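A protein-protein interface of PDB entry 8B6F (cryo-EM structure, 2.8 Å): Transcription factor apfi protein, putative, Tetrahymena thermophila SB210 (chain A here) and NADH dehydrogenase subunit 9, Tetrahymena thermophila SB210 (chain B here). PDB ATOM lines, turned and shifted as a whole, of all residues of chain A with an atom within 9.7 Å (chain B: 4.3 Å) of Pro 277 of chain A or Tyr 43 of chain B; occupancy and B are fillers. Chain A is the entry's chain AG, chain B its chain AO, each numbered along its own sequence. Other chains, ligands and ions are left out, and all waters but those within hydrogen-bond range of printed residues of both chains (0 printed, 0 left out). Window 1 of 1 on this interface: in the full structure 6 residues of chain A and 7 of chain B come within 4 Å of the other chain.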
ATOM      1  N   GLN A 274      11.540 -12.780   0.933  1.00  0.00           N
ATOM      2  CA  GLN A 274      10.706 -12.527  -0.230  1.00  0.00           C
ATOM      3  C   GLN A 274       9.613 -11.530   0.113  1.00  0.00           C
ATOM      4  O   GLN A 274       9.054 -11.553   1.214  1.00  0.00           O
ATOM      5  CB  GLN A 274      10.090 -13.829  -0.739  1.00  0.00           C
ATOM      6  CG  GLN A 274      11.127 -14.822  -1.219  1.00  0.00           C
ATOM      7  CD  GLN A 274      10.515 -16.013  -1.914  1.00  0.00           C
ATOM      8  OE1 GLN A 274       9.306 -16.231  -1.855  1.00  0.00           O
ATOM      9  NE2 GLN A 274      11.351 -16.793  -2.588  1.00  0.00           N
ATOM     10  N   LEU A 275       9.311 -10.655  -0.834  1.00  0.00           N
ATOM     11  CA  LEU A 275       8.316  -9.624  -0.598  1.00  0.00           C
ATOM     12  C   LEU A 275       6.956 -10.266  -0.335  1.00  0.00           C
ATOM     13  O   LEU A 275       6.524 -11.127  -1.113  1.00  0.00           O
ATOM     14  CB  LEU A 275       8.243  -8.684  -1.801  1.00  0.00           C
ATOM     15  CG  LEU A 275       9.496  -7.858  -2.091  1.00  0.00           C
ATOM     16  CD1 LEU A 275       9.366  -7.141  -3.421  1.00  0.00           C
ATOM     17  CD2 LEU A 275       9.750  -6.858  -0.975  1.00  0.00           C
ATOM     18  N   PRO A 276       6.253  -9.882   0.735  1.00  0.00           N
ATOM     19  CA  PRO A 276       4.968 -10.514   1.018  1.00  0.00           C
ATOM     20  C   PRO A 276       3.957 -10.196  -0.068  1.00  0.00           C
ATOM     21  O   PRO A 276       4.053  -9.155  -0.739  1.00  0.00           O
ATOM     22  CB  PRO A 276       4.559  -9.898   2.368  1.00  0.00           C
ATOM     23  CG  PRO A 276       5.286  -8.620   2.436  1.00  0.00           C
ATOM     24  CD  PRO A 276       6.587  -8.853   1.734  1.00  0.00           C
ATOM     25  N   PRO A 277       2.972 -11.067  -0.284  1.00  0.00           N
ATOM     26  CA  PRO A 277       1.990 -10.809  -1.342  1.00  0.00           C
ATOM     27  C   PRO A 277       1.218  -9.522  -1.098  1.00  0.00           C
ATOM     28  O   PRO A 277       0.944  -9.140   0.042  1.00  0.00           O
ATOM     29  CB  PRO A 277       1.064 -12.030  -1.276  1.00  0.00           C
ATOM     30  CG  PRO A 277       1.833 -13.071  -0.552  1.00  0.00           C
ATOM     31  CD  PRO A 277       2.712 -12.341   0.407  1.00  0.00           C
ATOM     32  N   LEU A 278       0.869  -8.850  -2.190  1.00  0.00           N
ATOM     33  CA  LEU A 278      -0.025  -7.707  -2.101  1.00  0.00           C
ATOM     34  C   LEU A 278      -1.385  -8.160  -1.589  1.00  0.00           C
ATOM     35  O   LEU A 278      -1.868  -9.239  -1.939  1.00  0.00           O
ATOM     36  CB  LEU A 278      -0.176  -7.039  -3.467  1.00  0.00           C
ATOM     37  CG  LEU A 278       1.116  -6.548  -4.121  1.00  0.00           C
ATOM     38  CD1 LEU A 278       0.877  -6.233  -5.584  1.00  0.00           C
ATOM     39  CD2 LEU A 278       1.653  -5.329  -3.394  1.00  0.00           C
ATOM     40  N   GLU A 279      -2.008  -7.329  -0.753  1.00  0.00           N
ATOM     41  CA  GLU A 279      -3.292  -7.708  -0.179  1.00  0.00           C
ATOM     42  C   GLU A 279      -4.381  -7.832  -1.235  1.00  0.00           C
ATOM     43  O   GLU A 279      -5.399  -8.483  -0.983  1.00  0.00           O
ATOM     44  CB  GLU A 279      -3.712  -6.703   0.891  1.00  0.00           C
ATOM     45  CG  GLU A 279      -4.812  -7.222   1.800  1.00  0.00           C
ATOM     46  CD  GLU A 279      -5.088  -6.296   2.962  1.00  0.00           C
ATOM     47  OE1 GLU A 279      -4.573  -5.161   2.946  1.00  0.00           O
ATOM     48  OE2 GLU A 279      -5.814  -6.704   3.894  1.00  0.00           O
ATOM     49  N   SER A 280      -4.194  -7.225  -2.409  1.00  0.00           N
ATOM     50  CA  SER A 280      -5.148  -7.404  -3.497  1.00  0.00           C
ATOM     51  C   SER A 280      -5.181  -8.840  -3.999  1.00  0.00           C
ATOM     52  O   SER A 280      -6.168  -9.242  -4.623  1.00  0.00           O
ATOM     53  CB  SER A 280      -4.808  -6.468  -4.657  1.00  0.00           C
ATOM     54  OG  SER A 280      -4.962  -5.110  -4.287  1.00  0.00           O
ATOM     55  N   GLU A 281      -4.126  -9.615  -3.748  1.00  0.00           N
ATOM     56  CA  GLU A 281      -4.089 -11.004  -4.179  1.00  0.00           C
ATOM     57  C   GLU A 281      -4.966 -11.907  -3.324  1.00  0.00           C
ATOM     58  O   GLU A 281      -5.158 -13.072  -3.685  1.00  0.00           O
ATOM     59  CB  GLU A 281      -2.649 -11.513  -4.155  1.00  0.00           C
ATOM     60  CG  GLU A 281      -1.695 -10.685  -5.002  1.00  0.00           C
ATOM     61  CD  GLU A 281      -0.271 -11.202  -4.954  1.00  0.00           C
ATOM     62  OE1 GLU A 281      -0.063 -12.323  -4.445  1.00  0.00           O
ATOM     63  OE2 GLU A 281       0.640 -10.488  -5.422  1.00  0.00           O
ATOM     64  N   PHE A 282      -5.487 -11.410  -2.206  1.00  0.00           N
ATOM     65  CA  PHE A 282      -6.374 -12.181  -1.348  1.00  0.00           C
ATOM     66  C   PHE A 282      -7.845 -11.935  -1.652  1.00  0.00           C
ATOM     67  O   PHE A 282      -8.705 -12.511  -0.978  1.00  0.00           O
ATOM     68  CB  PHE A 282      -6.105 -11.856   0.126  1.00  0.00           C
ATOM     69  CG  PHE A 282      -4.663 -11.987   0.531  1.00  0.00           C
ATOM     70  CD1 PHE A 282      -3.775 -12.745  -0.214  1.00  0.00           C
ATOM     71  CD2 PHE A 282      -4.199 -11.353   1.671  1.00  0.00           C
ATOM     72  CE1 PHE A 282      -2.451 -12.861   0.165  1.00  0.00           C
ATOM     73  CE2 PHE A 282      -2.877 -11.466   2.054  1.00  0.00           C
ATOM     74  CZ  PHE A 282      -2.003 -12.221   1.301  1.00  0.00           C
ATOM     75  N   TRP A 283      -8.155 -11.096  -2.640  1.00  0.00           N
ATOM     76  CA  TRP A 283      -9.525 -10.717  -2.956  1.00  0.00           C
ATOM     77  C   TRP A 283      -9.992 -11.258  -4.302  1.00  0.00           C
ATOM     78  O   TRP A 283     -11.078 -10.891  -4.760  1.00  0.00           O
ATOM     79  CB  TRP A 283      -9.663  -9.193  -2.938  1.00  0.00           C
ATOM     80  CG  TRP A 283      -9.227  -8.561  -1.652  1.00  0.00           C
ATOM     81  CD1 TRP A 283      -9.156  -9.158  -0.429  1.00  0.00           C
ATOM     82  CD2 TRP A 283      -8.794  -7.209  -1.466  1.00  0.00           C
ATOM     83  NE1 TRP A 283      -8.708  -8.261   0.510  1.00  0.00           N
ATOM     84  CE2 TRP A 283      -8.479  -7.057  -0.102  1.00  0.00           C
ATOM     85  CE3 TRP A 283      -8.644  -6.111  -2.320  1.00  0.00           C
ATOM     86  CZ2 TRP A 283      -8.022  -5.852   0.429  1.00  0.00           C
ATOM     87  CZ3 TRP A 283      -8.191  -4.914  -1.791  1.00  0.00           C
ATOM     88  CH2 TRP A 283      -7.887  -4.793  -0.428  1.00  0.00           C
ATOM     89  N   LYS A 284      -9.202 -12.111  -4.948  1.00  0.00           N
ATOM     90  CA  LYS A 284      -9.591 -12.639  -6.247  1.00  0.00           C
ATOM     91  C   LYS A 284     -10.909 -13.394  -6.141  1.00  0.00           C
ATOM     92  O   LYS A 284     -11.162 -14.104  -5.165  1.00  0.00           O
ATOM     93  CB  LYS A 284      -8.502 -13.559  -6.797  1.00  0.00           C
ATOM     94  CG  LYS A 284      -7.145 -12.894  -6.957  1.00  0.00           C
ATOM     95  CD  LYS A 284      -6.101 -13.887  -7.442  1.00  0.00           C
ATOM     96  CE  LYS A 284      -4.725 -13.244  -7.523  1.00  0.00           C
ATOM     97  NZ  LYS A 284      -3.671 -14.225  -7.910  1.00  0.00           N
ATOM     98  N   TYR A 287      -9.997 -18.856  -7.509  1.00  0.00           N
ATOM     99  CA  TYR A 287      -8.622 -19.323  -7.374  1.00  0.00           C
ATOM    100  C   TYR A 287      -8.394 -20.651  -8.085  1.00  0.00           C
ATOM    101  O   TYR A 287      -7.399 -21.330  -7.815  1.00  0.00           O
ATOM    102  CB  TYR A 287      -8.246 -19.452  -5.897  1.00  0.00           C
ATOM    103  CG  TYR A 287      -8.187 -18.132  -5.167  1.00  0.00           C
ATOM    104  CD1 TYR A 287      -7.056 -17.329  -5.236  1.00  0.00           C
ATOM    105  CD2 TYR A 287      -9.259 -17.690  -4.405  1.00  0.00           C
ATOM    106  CE1 TYR A 287      -6.996 -16.124  -4.572  1.00  0.00           C
ATOM    107  CE2 TYR A 287      -9.210 -16.486  -3.737  1.00  0.00           C
ATOM    108  CZ  TYR A 287      -8.076 -15.708  -3.824  1.00  0.00           C
ATOM    109  OH  TYR A 287      -8.021 -14.507  -3.158  1.00  0.00           O
ATOM    110  N   TRP B  41      -8.265  -5.496   9.147  1.00  0.00           N
ATOM    111  CA  TRP B  41      -7.157  -4.585   8.900  1.00  0.00           C
ATOM    112  C   TRP B  41      -5.837  -5.097   9.456  1.00  0.00           C
ATOM    113  O   TRP B  41      -4.809  -4.439   9.274  1.00  0.00           O
ATOM    114  CB  TRP B  41      -7.457  -3.211   9.508  1.00  0.00           C
ATOM    115  CG  TRP B  41      -8.586  -2.485   8.859  1.00  0.00           C
ATOM    116  CD1 TRP B  41      -9.895  -2.496   9.238  1.00  0.00           C
ATOM    117  CD2 TRP B  41      -8.505  -1.626   7.719  1.00  0.00           C
ATOM    118  NE1 TRP B  41     -10.635  -1.697   8.403  1.00  0.00           N
ATOM    119  CE2 TRP B  41      -9.804  -1.152   7.459  1.00  0.00           C
ATOM    120  CE3 TRP B  41      -7.458  -1.212   6.891  1.00  0.00           C
ATOM    121  CZ2 TRP B  41     -10.086  -0.285   6.407  1.00  0.00           C
ATOM    122  CZ3 TRP B  41      -7.737  -0.354   5.849  1.00  0.00           C
ATOM    123  CH2 TRP B  41      -9.041   0.103   5.614  1.00  0.00           C
ATOM    124  N   PHE B  42      -5.838  -6.251  10.128  1.00  0.00           N
ATOM    125  CA  PHE B  42      -4.621  -6.750  10.757  1.00  0.00           C
ATOM    126  C   PHE B  42      -3.498  -6.942   9.745  1.00  0.00           C
ATOM    127  O   PHE B  42      -2.350  -6.560  10.002  1.00  0.00           O
ATOM    128  CB  PHE B  42      -4.923  -8.060  11.485  1.00  0.00           C
ATOM    129  CG  PHE B  42      -3.758  -8.614  12.247  1.00  0.00           C
ATOM    130  CD1 PHE B  42      -3.322  -8.002  13.410  1.00  0.00           C
ATOM    131  CD2 PHE B  42      -3.113  -9.759  11.816  1.00  0.00           C
ATOM    132  CE1 PHE B  42      -2.256  -8.514  14.120  1.00  0.00           C
ATOM    133  CE2 PHE B  42      -2.047 -10.276  12.522  1.00  0.00           C
ATOM    134  CZ  PHE B  42      -1.618  -9.652  13.676  1.00  0.00           C
ATOM    135  N   TYR B  43      -3.800  -7.536   8.590  1.00  0.00           N
ATOM    136  CA  TYR B  43      -2.750  -7.825   7.616  1.00  0.00           C
ATOM    137  C   TYR B  43      -2.133  -6.546   7.062  1.00  0.00           C
ATOM    138  O   TYR B  43      -0.906  -6.423   6.981  1.00  0.00           O
ATOM    139  CB  TYR B  43      -3.303  -8.684   6.482  1.00  0.00           C
ATOM    140  CG  TYR B  43      -2.255  -9.063   5.464  1.00  0.00           C
ATOM    141  CD1 TYR B  43      -1.396 -10.130   5.687  1.00  0.00           C
ATOM    142  CD2 TYR B  43      -2.123  -8.353   4.280  1.00  0.00           C
ATOM    143  CE1 TYR B  43      -0.435 -10.478   4.761  1.00  0.00           C
ATOM    144  CE2 TYR B  43      -1.166  -8.692   3.347  1.00  0.00           C
ATOM    145  CZ  TYR B  43      -0.326  -9.755   3.592  1.00  0.00           C
ATOM    146  OH  TYR B  43       0.629 -10.095   2.664  1.00  0.00           O
ATOM    147  N   SER B  44      -2.968  -5.579   6.678  1.00  0.00           N
ATOM    148  CA  SER B  44      -2.448  -4.315   6.165  1.00  0.00           C
ATOM    149  C   SER B  44      -1.659  -3.571   7.234  1.00  0.00           C
ATOM    150  O   SER B  44      -0.637  -2.944   6.940  1.00  0.00           O
ATOM    151  CB  SER B  44      -3.593  -3.446   5.647  1.00  0.00           C
ATOM    152  OG  SER B  44      -4.497  -3.122   6.688  1.00  0.00           O
ATOM    153  N   ILE B  45      -2.118  -3.635   8.483  1.00  0.00           N
ATOM    154  CA  ILE B  45      -1.411  -2.968   9.571  1.00  0.00           C
ATOM    155  C   ILE B  45      -0.029  -3.577   9.758  1.00  0.00           C
ATOM    156  O   ILE B  45       0.955  -2.862   9.976  1.00  0.00           O
ATOM    157  CB  ILE B  45      -2.252  -3.027  10.859  1.00  0.00           C
ATOM    158  CG1 ILE B  45      -3.457  -2.097  10.711  1.00  0.00           C
ATOM    159  CG2 ILE B  45      -1.423  -2.667  12.082  1.00  0.00           C
ATOM    160  CD1 ILE B  45      -4.548  -2.364  11.685  1.00  0.00           C
ATOM    161  N   ASN B  46       0.071  -4.902   9.677  1.00  0.00           N
ATOM    162  CA  ASN B  46       1.378  -5.542   9.776  1.00  0.00           C
ATOM    163  C   ASN B  46       2.251  -5.192   8.580  1.00  0.00           C
ATOM    164  O   ASN B  46       3.469  -5.043   8.717  1.00  0.00           O
ATOM    165  CB  ASN B  46       1.214  -7.052   9.910  1.00  0.00           C
ATOM    166  CG  ASN B  46       0.861  -7.465  11.317  1.00  0.00           C
ATOM    167  OD1 ASN B  46       1.702  -7.969  12.058  1.00  0.00           O
ATOM    168  ND2 ASN B  46      -0.386  -7.233  11.703  1.00  0.00           N
ATOM    169  N   LEU B  47       1.652  -5.069   7.394  1.00  0.00           N
ATOM    170  CA  LEU B  47       2.417  -4.624   6.234  1.00  0.00           C
ATOM    171  C   LEU B  47       3.023  -3.250   6.486  1.00  0.00           C
ATOM    172  O   LEU B  47       4.197  -3.009   6.181  1.00  0.00           O
ATOM    173  CB  LEU B  47       1.525  -4.589   4.992  1.00  0.00           C
ATOM    174  CG  LEU B  47       1.337  -5.878   4.188  1.00  0.00           C
ATOM    175  CD1 LEU B  47       0.370  -5.631   3.043  1.00  0.00           C
ATOM    176  CD2 LEU B  47       2.656  -6.408   3.659  1.00  0.00           C
ATOM    177  N   ASP B 123      -6.486 -13.409   8.937  1.00  0.00           N
ATOM    178  CA  ASP B 123      -5.373 -13.446   7.999  1.00  0.00           C
ATOM    179  C   ASP B 123      -4.060 -13.656   8.740  1.00  0.00           C
ATOM    180  O   ASP B 123      -3.786 -12.989   9.743  1.00  0.00           O
ATOM    181  CB  ASP B 123      -5.312 -12.150   7.192  1.00  0.00           C
ATOM    182  CG  ASP B 123      -6.447 -12.026   6.201  1.00  0.00           C
ATOM    183  OD1 ASP B 123      -6.892 -13.065   5.673  1.00  0.00           O
ATOM    184  OD2 ASP B 123      -6.893 -10.888   5.947  1.00  0.00           O
ATOM    185  N   SER B 124      -3.248 -14.582   8.246  1.00  0.00           N
ATOM    186  CA  SER B 124      -1.936 -14.824   8.817  1.00  0.00           C
ATOM    187  C   SER B 124      -0.953 -13.743   8.374  1.00  0.00           C
ATOM    188  O   SER B 124      -1.124 -13.098   7.337  1.00  0.00           O
ATOM    189  CB  SER B 124      -1.422 -16.203   8.406  1.00  0.00           C
ATOM    190  OG  SER B 124      -0.097 -16.410   8.860  1.00  0.00           O
ATOM    191  N   ARG B 127       3.847 -14.454   6.356  1.00  0.00           N
ATOM    192  CA  ARG B 127       4.491 -13.989   5.138  1.00  0.00           C
ATOM    193  C   ARG B 127       5.161 -12.635   5.314  1.00  0.00           C
ATOM    194  O   ARG B 127       5.971 -12.249   4.466  1.00  0.00           O
ATOM    195  CB  ARG B 127       3.470 -13.915   4.002  1.00  0.00           C
ATOM    196  CG  ARG B 127       2.858 -15.259   3.653  1.00  0.00           C
ATOM    197  CD  ARG B 127       1.909 -15.154   2.474  1.00  0.00           C
ATOM    198  NE  ARG B 127       1.385 -16.458   2.091  1.00  0.00           N
ATOM    199  CZ  ARG B 127       2.022 -17.325   1.317  1.00  0.00           C
ATOM    200  NH1 ARG B 127       3.219 -17.060   0.821  1.00  0.00           N
ATOM    201  NH2 ARG B 127       1.446 -18.490   1.036  1.00  0.00           N
ATOM    202  N   ILE B 128       4.848 -11.914   6.384  1.00  0.00           N
ATOM    203  CA  ILE B 128       5.484 -10.639   6.694  1.00  0.00           C
ATOM    204  C   ILE B 128       6.555 -10.803   7.763  1.00  0.00           C
ATOM    205  O   ILE B 128       7.664 -10.290   7.624  1.00  0.00           O
ATOM    206  CB  ILE B 128       4.421  -9.603   7.121  1.00  0.00           C
ATOM    207  CG1 ILE B 128       3.304  -9.530   6.075  1.00  0.00           C
ATOM    208  CG2 ILE B 128       5.068  -8.239   7.315  1.00  0.00           C
ATOM    209  CD1 ILE B 128       2.163  -8.617   6.449  1.00  0.00           C
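OH of Tyr 43 of chain B sits at hydrogen-bond distance from O of Pro 277 of chain A, at 2.8 Å.
O of Phe 282 of chain A sits close to OH of Tyr 287 of chain A, 3.0 Å away.
O of Trp 41 of chain B is in hydrogen-bond range of OG of Ser 44 of chain B, 2.9 Å away.
Among the printed residues, merely in contact across the chains: Pro 276 of chain A with Tyr 43 of chain B (3.9 Å), Pro 276 of chain A with Leu 47 of chain B (3.6 Å), Pro 276 of chain A with Arg 127 of chain B (3.5 Å), Pro 276 of chain A with Ile 128 of chain B (3.9 Å), Pro 277 of chain A with Arg 127 of chain B (3.6 Å), Glu 279 of chain A with Tyr 43 of chain B (3.8 Å), Glu 279 of chain A with Ser 44 of chain B (3.3 Å) and Phe 282 of chain A with Tyr 43 of chain B (3.4 Å).
Of the printed residues of chain B, Pro 277 of chain A touches Tyr 43 (2.8 Å) and Arg 127 (3.6 Å).
Printed residues of chain A within 4 Å of Tyr 43 of chain B: Pro 276, Pro 277, Glu 279 and Phe 282.
Printed residues of chain B within 4 Å of Glu 279 of chain A: Tyr 43 (3.8 Å) and Ser 44 (3.3 Å).
Of the printed residues of chain A, Leu 47 of chain B touches Pro 276 (3.6 Å).
Of the printed residues of chain A, Ile 128 of chain B touches Pro 276 (3.9 Å).
Printed residues of chain B within 4 Å of Phe 282 of chain A: Tyr 43 (3.4 Å).
Ser 280 of chain A touches none of the printed residues of chain B.
Leu 278 of chain A touches none of the printed residues of chain B.
The nearest residue of chain A that does not touch Tyr 43 of chain B is Leu 278 of chain A (5.0 Å).
Of the 12 printed residues of chain A, 4 touch a printed residue of chain B.
Hydrophobic or aromatic side chains of chain A that line the printed part of chain B: Pro 276, Pro 277 and Phe 282.
Along chain A the printed residues that touch a printed residue of chain B span positions 276 to 282.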
